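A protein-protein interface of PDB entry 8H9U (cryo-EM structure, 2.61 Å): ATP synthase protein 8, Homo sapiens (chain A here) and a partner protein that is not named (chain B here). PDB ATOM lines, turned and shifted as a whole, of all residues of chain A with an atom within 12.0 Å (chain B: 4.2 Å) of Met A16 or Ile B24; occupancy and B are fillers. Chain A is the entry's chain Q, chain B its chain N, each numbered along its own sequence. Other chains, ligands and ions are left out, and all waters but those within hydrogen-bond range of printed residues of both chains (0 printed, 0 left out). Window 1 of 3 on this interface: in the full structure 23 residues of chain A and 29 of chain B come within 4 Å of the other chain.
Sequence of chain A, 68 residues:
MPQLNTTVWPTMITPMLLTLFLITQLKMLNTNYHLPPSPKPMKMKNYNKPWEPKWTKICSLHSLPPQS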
ATOM      1  N   VAL A   8     -24.290   9.275  22.447  1.00  0.00           N
ATOM      2  CA  VAL A   8     -23.323   9.945  23.310  1.00  0.00           C
ATOM      3  C   VAL A   8     -23.630  11.429  23.379  1.00  0.00           C
ATOM      4  O   VAL A   8     -22.865  12.202  23.964  1.00  0.00           O
ATOM      5  CB  VAL A   8     -21.884   9.721  22.820  1.00  0.00           C
ATOM      6  CG1 VAL A   8     -21.555   8.247  22.806  1.00  0.00           C
ATOM      7  CG2 VAL A   8     -21.714  10.322  21.444  1.00  0.00           C
ATOM      8  N   TRP A   9     -24.734  11.844  22.765  1.00  0.00           N
ATOM      9  CA  TRP A   9     -25.147  13.239  22.879  1.00  0.00           C
ATOM     10  C   TRP A   9     -25.221  13.699  24.329  1.00  0.00           C
ATOM     11  O   TRP A   9     -24.685  14.778  24.633  1.00  0.00           O
ATOM     12  CB  TRP A   9     -26.471  13.450  22.140  1.00  0.00           C
ATOM     13  CG  TRP A   9     -26.296  13.661  20.668  1.00  0.00           C
ATOM     14  CD1 TRP A   9     -25.248  13.249  19.904  1.00  0.00           C
ATOM     15  CD2 TRP A   9     -27.193  14.340  19.783  1.00  0.00           C
ATOM     16  NE1 TRP A   9     -25.434  13.626  18.599  1.00  0.00           N
ATOM     17  CE2 TRP A   9     -26.623  14.298  18.499  1.00  0.00           C
ATOM     18  CE3 TRP A   9     -28.423  14.979  19.953  1.00  0.00           C
ATOM     19  CZ2 TRP A   9     -27.237  14.867  17.392  1.00  0.00           C
ATOM     20  CZ3 TRP A   9     -29.031  15.543  18.852  1.00  0.00           C
ATOM     21  CH2 TRP A   9     -28.439  15.484  17.588  1.00  0.00           C
ATOM     22  N   PRO A  10     -25.811  12.948  25.270  1.00  0.00           N
ATOM     23  CA  PRO A  10     -25.814  13.420  26.666  1.00  0.00           C
ATOM     24  C   PRO A  10     -24.428  13.596  27.263  1.00  0.00           C
ATOM     25  O   PRO A  10     -24.285  14.265  28.292  1.00  0.00           O
ATOM     26  CB  PRO A  10     -26.608  12.331  27.398  1.00  0.00           C
ATOM     27  CG  PRO A  10     -27.468  11.736  26.355  1.00  0.00           C
ATOM     28  CD  PRO A  10     -26.632  11.733  25.118  1.00  0.00           C
ATOM     29  N   THR A  11     -23.399  13.010  26.655  1.00  0.00           N
ATOM     30  CA  THR A  11     -22.044  13.215  27.152  1.00  0.00           C
ATOM     31  C   THR A  11     -21.472  14.556  26.703  1.00  0.00           C
ATOM     32  O   THR A  11     -20.534  15.060  27.326  1.00  0.00           O
ATOM     33  CB  THR A  11     -21.157  12.052  26.701  1.00  0.00           C
ATOM     34  OG1 THR A  11     -21.650  10.838  27.275  1.00  0.00           O
ATOM     35  CG2 THR A  11     -19.718  12.241  27.141  1.00  0.00           C
ATOM     36  N   MET A  12     -22.029  15.158  25.654  1.00  0.00           N
ATOM     37  CA  MET A  12     -21.617  16.495  25.248  1.00  0.00           C
ATOM     38  C   MET A  12     -22.512  17.583  25.814  1.00  0.00           C
ATOM     39  O   MET A  12     -22.018  18.660  26.160  1.00  0.00           O
ATOM     40  CB  MET A  12     -21.614  16.619  23.725  1.00  0.00           C
ATOM     41  CG  MET A  12     -20.869  15.527  23.013  1.00  0.00           C
ATOM     42  SD  MET A  12     -19.132  15.503  23.449  1.00  0.00           S
ATOM     43  CE  MET A  12     -18.659  13.974  22.668  1.00  0.00           C
ATOM     44  N   ILE A  13     -23.815  17.333  25.902  1.00  0.00           N
ATOM     45  CA  ILE A  13     -24.734  18.372  26.342  1.00  0.00           C
ATOM     46  C   ILE A  13     -24.420  18.815  27.763  1.00  0.00           C
ATOM     47  O   ILE A  13     -24.368  20.014  28.047  1.00  0.00           O
ATOM     48  CB  ILE A  13     -26.191  17.897  26.212  1.00  0.00           C
ATOM     49  CG1 ILE A  13     -26.436  17.224  24.861  1.00  0.00           C
ATOM     50  CG2 ILE A  13     -27.146  19.053  26.415  1.00  0.00           C
ATOM     51  CD1 ILE A  13     -26.089  18.073  23.681  1.00  0.00           C
ATOM     52  N   THR A  14     -24.197  17.870  28.683  1.00  0.00           N
ATOM     53  CA  THR A  14     -24.083  18.260  30.088  1.00  0.00           C
ATOM     54  C   THR A  14     -22.808  19.042  30.391  1.00  0.00           C
ATOM     55  O   THR A  14     -22.915  20.144  30.955  1.00  0.00           O
ATOM     56  CB  THR A  14     -24.246  17.036  30.996  1.00  0.00           C
ATOM     57  OG1 THR A  14     -23.049  16.251  31.009  1.00  0.00           O
ATOM     58  CG2 THR A  14     -25.411  16.181  30.535  1.00  0.00           C
ATOM     59  N   PRO A  15     -21.600  18.576  30.048  1.00  0.00           N
ATOM     60  CA  PRO A  15     -20.413  19.314  30.498  1.00  0.00           C
ATOM     61  C   PRO A  15     -20.254  20.658  29.819  1.00  0.00           C
ATOM     62  O   PRO A  15     -19.640  21.558  30.401  1.00  0.00           O
ATOM     63  CB  PRO A  15     -19.263  18.365  30.157  1.00  0.00           C
ATOM     64  CG  PRO A  15     -19.723  17.692  28.965  1.00  0.00           C
ATOM     65  CD  PRO A  15     -21.220  17.534  29.083  1.00  0.00           C
ATOM     66  N   MET A  16     -20.776  20.827  28.605  1.00  0.00           N
ATOM     67  CA  MET A  16     -20.862  22.163  28.030  1.00  0.00           C
ATOM     68  C   MET A  16     -21.683  23.076  28.925  1.00  0.00           C
ATOM     69  O   MET A  16     -21.247  24.175  29.285  1.00  0.00           O
ATOM     70  CB  MET A  16     -21.466  22.099  26.630  1.00  0.00           C
ATOM     71  CG  MET A  16     -21.498  23.428  25.913  1.00  0.00           C
ATOM     72  SD  MET A  16     -22.924  24.435  26.342  1.00  0.00           S
ATOM     73  CE  MET A  16     -24.240  23.396  25.741  1.00  0.00           C
ATOM     74  N   LEU A  17     -22.890  22.637  29.286  1.00  0.00           N
ATOM     75  CA  LEU A  17     -23.711  23.405  30.212  1.00  0.00           C
ATOM     76  C   LEU A  17     -22.975  23.639  31.521  1.00  0.00           C
ATOM     77  O   LEU A  17     -23.145  24.682  32.161  1.00  0.00           O
ATOM     78  CB  LEU A  17     -25.033  22.682  30.454  1.00  0.00           C
ATOM     79  CG  LEU A  17     -25.882  22.486  29.202  1.00  0.00           C
ATOM     80  CD1 LEU A  17     -27.030  21.537  29.476  1.00  0.00           C
ATOM     81  CD2 LEU A  17     -26.391  23.815  28.692  1.00  0.00           C
ATOM     82  N   LEU A  18     -22.140  22.686  31.926  1.00  0.00           N
ATOM     83  CA  LEU A  18     -21.335  22.858  33.124  1.00  0.00           C
ATOM     84  C   LEU A  18     -20.141  23.771  32.887  1.00  0.00           C
ATOM     85  O   LEU A  18     -19.436  24.110  33.840  1.00  0.00           O
ATOM     86  CB  LEU A  18     -20.863  21.495  33.623  1.00  0.00           C
ATOM     87  CG  LEU A  18     -20.265  21.406  35.023  1.00  0.00           C
ATOM     88  CD1 LEU A  18     -21.286  21.850  36.049  1.00  0.00           C
ATOM     89  CD2 LEU A  18     -19.800  19.991  35.297  1.00  0.00           C
ATOM     90  N   THR A  19     -19.901  24.176  31.645  1.00  0.00           N
ATOM     91  CA  THR A  19     -18.767  25.024  31.305  1.00  0.00           C
ATOM     92  C   THR A  19     -19.183  26.362  30.722  1.00  0.00           C
ATOM     93  O   THR A  19     -18.652  27.401  31.120  1.00  0.00           O
ATOM     94  CB  THR A  19     -17.855  24.304  30.313  1.00  0.00           C
ATOM     95  OG1 THR A  19     -17.032  23.367  31.013  1.00  0.00           O
ATOM     96  CG2 THR A  19     -16.981  25.283  29.587  1.00  0.00           C
ATOM     97  N   LEU A  20     -20.124  26.364  29.786  1.00  0.00           N
ATOM     98  CA  LEU A  20     -20.587  27.620  29.225  1.00  0.00           C
ATOM     99  C   LEU A  20     -21.459  28.391  30.202  1.00  0.00           C
ATOM    100  O   LEU A  20     -21.425  29.625  30.215  1.00  0.00           O
ATOM    101  CB  LEU A  20     -21.352  27.358  27.933  1.00  0.00           C
ATOM    102  CG  LEU A  20     -22.041  28.576  27.343  1.00  0.00           C
ATOM    103  CD1 LEU A  20     -20.996  29.542  26.864  1.00  0.00           C
ATOM    104  CD2 LEU A  20     -22.960  28.171  26.220  1.00  0.00           C
ATOM    105  N   PHE A  21     -22.231  27.693  31.038  1.00  0.00           N
ATOM    106  CA  PHE A  21     -23.225  28.346  31.875  1.00  0.00           C
ATOM    107  C   PHE A  21     -22.827  28.481  33.333  1.00  0.00           C
ATOM    108  O   PHE A  21     -23.440  29.283  34.040  1.00  0.00           O
ATOM    109  CB  PHE A  21     -24.561  27.596  31.802  1.00  0.00           C
ATOM    110  CG  PHE A  21     -25.379  27.949  30.606  1.00  0.00           C
ATOM    111  CD1 PHE A  21     -26.083  29.132  30.560  1.00  0.00           C
ATOM    112  CD2 PHE A  21     -25.444  27.099  29.523  1.00  0.00           C
ATOM    113  CE1 PHE A  21     -26.835  29.457  29.459  1.00  0.00           C
ATOM    114  CE2 PHE A  21     -26.195  27.422  28.418  1.00  0.00           C
ATOM    115  CZ  PHE A  21     -26.889  28.602  28.386  1.00  0.00           C
ATOM    116  N   LEU A  22     -21.846  27.720  33.813  1.00  0.00           N
ATOM    117  CA  LEU A  22     -21.426  27.849  35.203  1.00  0.00           C
ATOM    118  C   LEU A  22     -19.982  28.311  35.339  1.00  0.00           C
ATOM    119  O   LEU A  22     -19.734  29.344  35.961  1.00  0.00           O
ATOM    120  CB  LEU A  22     -21.635  26.523  35.944  1.00  0.00           C
ATOM    121  CG  LEU A  22     -21.496  26.551  37.466  1.00  0.00           C
ATOM    122  CD1 LEU A  22     -22.460  25.565  38.089  1.00  0.00           C
ATOM    123  CD2 LEU A  22     -20.079  26.234  37.903  1.00  0.00           C
ATOM    124  N   ILE A  23     -19.022  27.589  34.769  1.00  0.00           N
ATOM    125  CA  ILE A  23     -17.624  27.835  35.102  1.00  0.00           C
ATOM    126  C   ILE A  23     -17.117  29.107  34.442  1.00  0.00           C
ATOM    127  O   ILE A  23     -16.656  30.028  35.121  1.00  0.00           O
ATOM    128  CB  ILE A  23     -16.760  26.626  34.720  1.00  0.00           C
ATOM    129  CG1 ILE A  23     -17.093  25.440  35.615  1.00  0.00           C
ATOM    130  CG2 ILE A  23     -15.301  26.975  34.851  1.00  0.00           C
ATOM    131  CD1 ILE A  23     -16.333  24.195  35.265  1.00  0.00           C
ATOM    132  N   THR A  24     -17.171  29.169  33.112  1.00  0.00           N
ATOM    133  CA  THR A  24     -16.649  30.336  32.409  1.00  0.00           C
ATOM    134  C   THR A  24     -17.332  31.612  32.872  1.00  0.00           C
ATOM    135  O   THR A  24     -16.673  32.633  33.092  1.00  0.00           O
ATOM    136  CB  THR A  24     -16.815  30.161  30.907  1.00  0.00           C
ATOM    137  OG1 THR A  24     -16.466  28.822  30.547  1.00  0.00           O
ATOM    138  CG2 THR A  24     -15.911  31.118  30.175  1.00  0.00           C
ATOM    139  N   GLN A  25     -18.656  31.577  33.022  1.00  0.00           N
ATOM    140  CA  GLN A  25     -19.357  32.720  33.589  1.00  0.00           C
ATOM    141  C   GLN A  25     -18.793  33.083  34.953  1.00  0.00           C
ATOM    142  O   GLN A  25     -18.663  34.265  35.284  1.00  0.00           O
ATOM    143  CB  GLN A  25     -20.847  32.416  33.691  1.00  0.00           C
ATOM    144  CG  GLN A  25     -21.533  32.273  32.360  1.00  0.00           C
ATOM    145  CD  GLN A  25     -22.972  32.711  32.419  1.00  0.00           C
ATOM    146  OE1 GLN A  25     -23.564  32.797  33.493  1.00  0.00           O
ATOM    147  NE2 GLN A  25     -23.547  33.002  31.262  1.00  0.00           N
ATOM    148  N   LEU A  26     -18.426  32.078  35.745  1.00  0.00           N
ATOM    149  CA  LEU A  26     -17.907  32.340  37.079  1.00  0.00           C
ATOM    150  C   LEU A  26     -16.507  32.934  37.027  1.00  0.00           C
ATOM    151  O   LEU A  26     -15.995  33.404  38.046  1.00  0.00           O
ATOM    152  CB  LEU A  26     -17.927  31.048  37.892  1.00  0.00           C
ATOM    153  CG  LEU A  26     -17.681  31.092  39.391  1.00  0.00           C
ATOM    154  CD1 LEU A  26     -18.665  30.183  40.089  1.00  0.00           C
ATOM    155  CD2 LEU A  26     -16.261  30.655  39.674  1.00  0.00           C
ATOM    156  N   LYS A  27     -15.876  32.931  35.855  1.00  0.00           N
ATOM    157  CA  LYS A  27     -14.581  33.581  35.720  1.00  0.00           C
ATOM    158  C   LYS A  27     -14.708  34.990  35.167  1.00  0.00           C
ATOM    159  O   LYS A  27     -13.833  35.825  35.411  1.00  0.00           O
ATOM    160  CB  LYS A  27     -13.662  32.749  34.832  1.00  0.00           C
ATOM    161  CG  LYS A  27     -13.085  31.547  35.536  1.00  0.00           C
ATOM    162  CD  LYS A  27     -12.215  30.735  34.613  1.00  0.00           C
ATOM    163  CE  LYS A  27     -11.863  29.409  35.244  1.00  0.00           C
ATOM    164  NZ  LYS A  27     -11.150  29.592  36.533  1.00  0.00           N
ATOM    165  N   ALA B  20     -14.636  12.999  26.858  1.00  0.00           N
ATOM    166  CA  ALA B  20     -15.161  14.245  26.318  1.00  0.00           C
ATOM    167  C   ALA B  20     -15.596  15.197  27.421  1.00  0.00           C
ATOM    168  O   ALA B  20     -15.647  16.412  27.203  1.00  0.00           O
ATOM    169  CB  ALA B  20     -16.329  13.960  25.379  1.00  0.00           C
ATOM    170  N   VAL B  21     -15.917  14.676  28.606  1.00  0.00           N
ATOM    171  CA  VAL B  21     -16.350  15.546  29.696  1.00  0.00           C
ATOM    172  C   VAL B  21     -15.176  16.354  30.226  1.00  0.00           C
ATOM    173  O   VAL B  21     -15.351  17.437  30.792  1.00  0.00           O
ATOM    174  CB  VAL B  21     -17.024  14.727  30.811  1.00  0.00           C
ATOM    175  CG1 VAL B  21     -18.060  13.789  30.223  1.00  0.00           C
ATOM    176  CG2 VAL B  21     -15.990  13.961  31.618  1.00  0.00           C
ATOM    177  N   LEU B  22     -13.958  15.844  30.047  1.00  0.00           N
ATOM    178  CA  LEU B  22     -12.788  16.606  30.465  1.00  0.00           C
ATOM    179  C   LEU B  22     -12.465  17.699  29.457  1.00  0.00           C
ATOM    180  O   LEU B  22     -12.196  18.844  29.836  1.00  0.00           O
ATOM    181  CB  LEU B  22     -11.593  15.674  30.649  1.00  0.00           C
ATOM    182  CG  LEU B  22     -10.293  16.279  31.181  1.00  0.00           C
ATOM    183  CD1 LEU B  22      -9.536  15.223  31.959  1.00  0.00           C
ATOM    184  CD2 LEU B  22      -9.416  16.841  30.070  1.00  0.00           C
ATOM    185  N   ILE B  23     -12.490  17.363  28.168  1.00  0.00           N
ATOM    186  CA  ILE B  23     -12.075  18.308  27.138  1.00  0.00           C
ATOM    187  C   ILE B  23     -13.012  19.502  27.077  1.00  0.00           C
ATOM    188  O   ILE B  23     -12.589  20.617  26.758  1.00  0.00           O
ATOM    189  CB  ILE B  23     -11.984  17.589  25.784  1.00  0.00           C
ATOM    190  CG1 ILE B  23     -11.017  16.415  25.883  1.00  0.00           C
ATOM    191  CG2 ILE B  23     -11.548  18.542  24.704  1.00  0.00           C
ATOM    192  CD1 ILE B  23     -10.787  15.723  24.580  1.00  0.00           C
ATOM    193  N   ILE B  24     -14.291  19.304  27.381  1.00  0.00           N
ATOM    194  CA  ILE B  24     -15.207  20.431  27.359  1.00  0.00           C
ATOM    195  C   ILE B  24     -15.042  21.288  28.607  1.00  0.00           C
ATOM    196  O   ILE B  24     -15.267  22.501  28.565  1.00  0.00           O
ATOM    197  CB  ILE B  24     -16.647  19.927  27.191  1.00  0.00           C
ATOM    198  CG1 ILE B  24     -16.760  19.111  25.906  1.00  0.00           C
ATOM    199  CG2 ILE B  24     -17.612  21.086  27.151  1.00  0.00           C
ATOM    200  CD1 ILE B  24     -18.173  18.899  25.435  1.00  0.00           C
ATOM    201  N   LEU B  25     -14.633  20.688  29.727  1.00  0.00           N
ATOM    202  CA  LEU B  25     -14.378  21.448  30.946  1.00  0.00           C
ATOM    203  C   LEU B  25     -13.028  22.152  30.931  1.00  0.00           C
ATOM    204  O   LEU B  25     -12.756  22.959  31.823  1.00  0.00           O
ATOM    205  CB  LEU B  25     -14.442  20.533  32.169  1.00  0.00           C
ATOM    206  CG  LEU B  25     -15.780  19.950  32.620  1.00  0.00           C
ATOM    207  CD1 LEU B  25     -15.546  18.919  33.709  1.00  0.00           C
ATOM    208  CD2 LEU B  25     -16.715  21.030  33.114  1.00  0.00           C
ATOM    209  N   PHE B  26     -12.182  21.867  29.942  1.00  0.00           N
ATOM    210  CA  PHE B  26     -10.810  22.373  29.989  1.00  0.00           C
ATOM    211  C   PHE B  26     -10.683  23.840  29.598  1.00  0.00           C
ATOM    212  O   PHE B  26     -10.026  24.588  30.338  1.00  0.00           O
ATOM    213  CB  PHE B  26      -9.904  21.493  29.130  1.00  0.00           C
ATOM    214  CG  PHE B  26      -8.465  21.886  29.184  1.00  0.00           C
ATOM    215  CD1 PHE B  26      -7.624  21.339  30.130  1.00  0.00           C
ATOM    216  CD2 PHE B  26      -7.951  22.803  28.293  1.00  0.00           C
ATOM    217  CE1 PHE B  26      -6.300  21.700  30.182  1.00  0.00           C
ATOM    218  CE2 PHE B  26      -6.630  23.166  28.344  1.00  0.00           C
ATOM    219  CZ  PHE B  26      -5.805  22.613  29.288  1.00  0.00           C
ATOM    220  N   PRO B  27     -11.229  24.312  28.475  1.00  0.00           N
ATOM    221  CA  PRO B  27     -10.894  25.667  27.981  1.00  0.00           C
ATOM    222  C   PRO B  27     -10.997  26.749  29.045  1.00  0.00           C
ATOM    223  O   PRO B  27     -10.162  27.665  29.057  1.00  0.00           O
ATOM    224  CB  PRO B  27     -11.912  25.886  26.854  1.00  0.00           C
ATOM    225  CG  PRO B  27     -12.135  24.539  26.328  1.00  0.00           C
ATOM    226  CD  PRO B  27     -12.107  23.616  27.515  1.00  0.00           C
ATOM    227  N   PHE B  78     -15.662  31.068  25.185  1.00  0.00           N
ATOM    228  CA  PHE B  78     -15.647  29.611  25.238  1.00  0.00           C
ATOM    229  C   PHE B  78     -15.561  29.013  23.842  1.00  0.00           C
ATOM    230  O   PHE B  78     -14.801  28.068  23.606  1.00  0.00           O
ATOM    231  CB  PHE B  78     -16.886  29.096  25.960  1.00  0.00           C
ATOM    232  CG  PHE B  78     -17.117  27.636  25.775  1.00  0.00           C
ATOM    233  CD1 PHE B  78     -16.260  26.717  26.332  1.00  0.00           C
ATOM    234  CD2 PHE B  78     -18.190  27.180  25.046  1.00  0.00           C
ATOM    235  CE1 PHE B  78     -16.467  25.376  26.163  1.00  0.00           C
ATOM    236  CE2 PHE B  78     -18.400  25.840  24.879  1.00  0.00           C
ATOM    237  CZ  PHE B  78     -17.537  24.937  25.440  1.00  0.00           C
ATOM    238  N   PRO B  94     -14.952  19.764  20.447  1.00  0.00           N
ATOM    239  CA  PRO B  94     -16.374  19.564  20.745  1.00  0.00           C
ATOM    240  C   PRO B  94     -17.300  20.536  20.041  1.00  0.00           C
ATOM    241  O   PRO B  94     -18.519  20.399  20.189  1.00  0.00           O
ATOM    242  CB  PRO B  94     -16.437  19.737  22.263  1.00  0.00           C
ATOM    243  CG  PRO B  94     -15.305  20.600  22.573  1.00  0.00           C
ATOM    244  CD  PRO B  94     -14.213  20.222  21.629  1.00  0.00           C
ATOM    245  N   MET B 100     -23.487  19.228  20.819  1.00  0.00           N
ATOM    246  CA  MET B 100     -23.118  20.360  21.655  1.00  0.00           C
ATOM    247  C   MET B 100     -23.573  21.678  21.043  1.00  0.00           C
ATOM    248  O   MET B 100     -24.233  22.481  21.710  1.00  0.00           O
ATOM    249  CB  MET B 100     -21.611  20.358  21.885  1.00  0.00           C
ATOM    250  CG  MET B 100     -21.066  21.660  22.395  1.00  0.00           C
ATOM    251  SD  MET B 100     -19.404  21.460  23.035  1.00  0.00           S
ATOM    252  CE  MET B 100     -18.746  23.084  22.709  1.00  0.00           C
ATOM    253  N   ALA B 103     -26.983  22.307  21.579  1.00  0.00           N
ATOM    254  CA  ALA B 103     -27.242  22.642  22.970  1.00  0.00           C
ATOM    255  C   ALA B 103     -26.739  24.025  23.352  1.00  0.00           C
ATOM    256  O   ALA B 103     -27.041  24.488  24.455  1.00  0.00           O
ATOM    257  CB  ALA B 103     -26.617  21.595  23.881  1.00  0.00           C
ATOM    258  N   MET B 104     -25.978  24.688  22.485  1.00  0.00           N
ATOM    259  CA  MET B 104     -25.619  26.083  22.701  1.00  0.00           C
ATOM    260  C   MET B 104     -26.521  27.035  21.939  1.00  0.00           C
ATOM    261  O   MET B 104     -26.771  28.148  22.408  1.00  0.00           O
ATOM    262  CB  MET B 104     -24.174  26.344  22.275  1.00  0.00           C
ATOM    263  CG  MET B 104     -23.136  25.814  23.222  1.00  0.00           C
ATOM    264  SD  MET B 104     -21.513  26.516  22.915  1.00  0.00           S
ATOM    265  CE  MET B 104     -21.255  26.004  21.228  1.00  0.00           C
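Of chain B, only Ile B24, Met B100, Ala B103 and Met B104 come within 4 Å of Met A16. Ile B24 touches just these residues of chain A: Met A12, Pro A15, Met A16 and Thr A19. Ala B20 touches just one residue of chain A: Met A12. Of chain A, only Thr A11 (3.8 Å) comes within 4 Å of Val B21. No residue of chain A comes within 4 Å of Leu B22. No residue of chain A comes within 4 Å of Ile B23. Of chain A, only Leu A18 (3.9 Å), Thr A19 (3.2 Å) and Ile A23 (3.8 Å) come within 4 Å of Leu B25. No residue of chain A comes within 4 Å of Pro B27. No residue of chain A comes within 4 Å of Pro B94. Met B100 touches just one residue of chain A: Met A16. Ala B103 touches just these residues of chain A: Ile A13 and Met A16. Met B104 touches two residues of chain A. Of the printed residues of chain B, Leu A20 touches Met B104 (3.8 Å). Of the printed residues of chain B, Thr A19 touches Ile B24, Leu B25 and Phe B78. Trp A9 touches none of the printed residues of chain B. The nearest residue of chain B that does not touch Met A16 is Phe B78 (4.1 Å). The nearest residue of chain A that does not touch Ile B24 is Thr A11 (4.9 Å). The nearest printed residue of chain A that does not touch Phe B78 is Met A16 (4.1 Å).
The side-chain hydroxyl of Thr A19 sits at hydrogen-bond distance from the backbone carbonyl oxygen of Ile B24 (3.1 Å).
The backbone carbonyl oxygen (O) of Pro A15 is in hydrogen-bond range of the side-chain hydroxyl (OG1) of Thr A19 (3.2 Å). The side-chain hydroxyl (OG1) of Thr A24 lies within hydrogen-bond range of the backbone carbonyl oxygen (O) of Thr A19 (2.7 Å).
Among the printed residues, merely in contact across the chains: Thr A19 with Leu B25 (3.2 Å), Met A16 with Ala B103 (3.3 Å), Met A16 with Met B104 (3.4 Å), Thr A19 with Phe B78 (3.5 Å), Met A16 with Ile B24 (3.5 Å), Ile A13 with Ala B103 (3.6 Å), Met A12 with Ala B20 (3.6 Å), Pro A15 with Ile B24 (3.8 Å), Leu A20 with Met B104 (3.8 Å), Thr A11 with Val B21 (3.8 Å), Ile A23 with Leu B25 (3.8 Å), Leu A18 with Leu B25 (3.9 Å), Met A12 with Ile B24 (3.9 Å) and Met A16 with Met B100 (3.96 Å).
Hydrophobic or aromatic side chains of chain A within 4 Å of the printed part of chain B: Met A12, Ile A13, Met A16, Leu A18, Leu A20 and Ile A23. Of the 13 printed residues of chain B, 8 touch a printed residue of chain A. Hydrophobic or aromatic side chains of chain B that line the printed part of chain A: Ala B20, Val B21, Ile B24, Leu B25, Phe B78, Met B100, Ala B103 and Met B104. Among the printed residues, no Asp or Glu carboxylate lies within 4 Å of a Lys or Arg side-chain nitrogen of the other chain.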
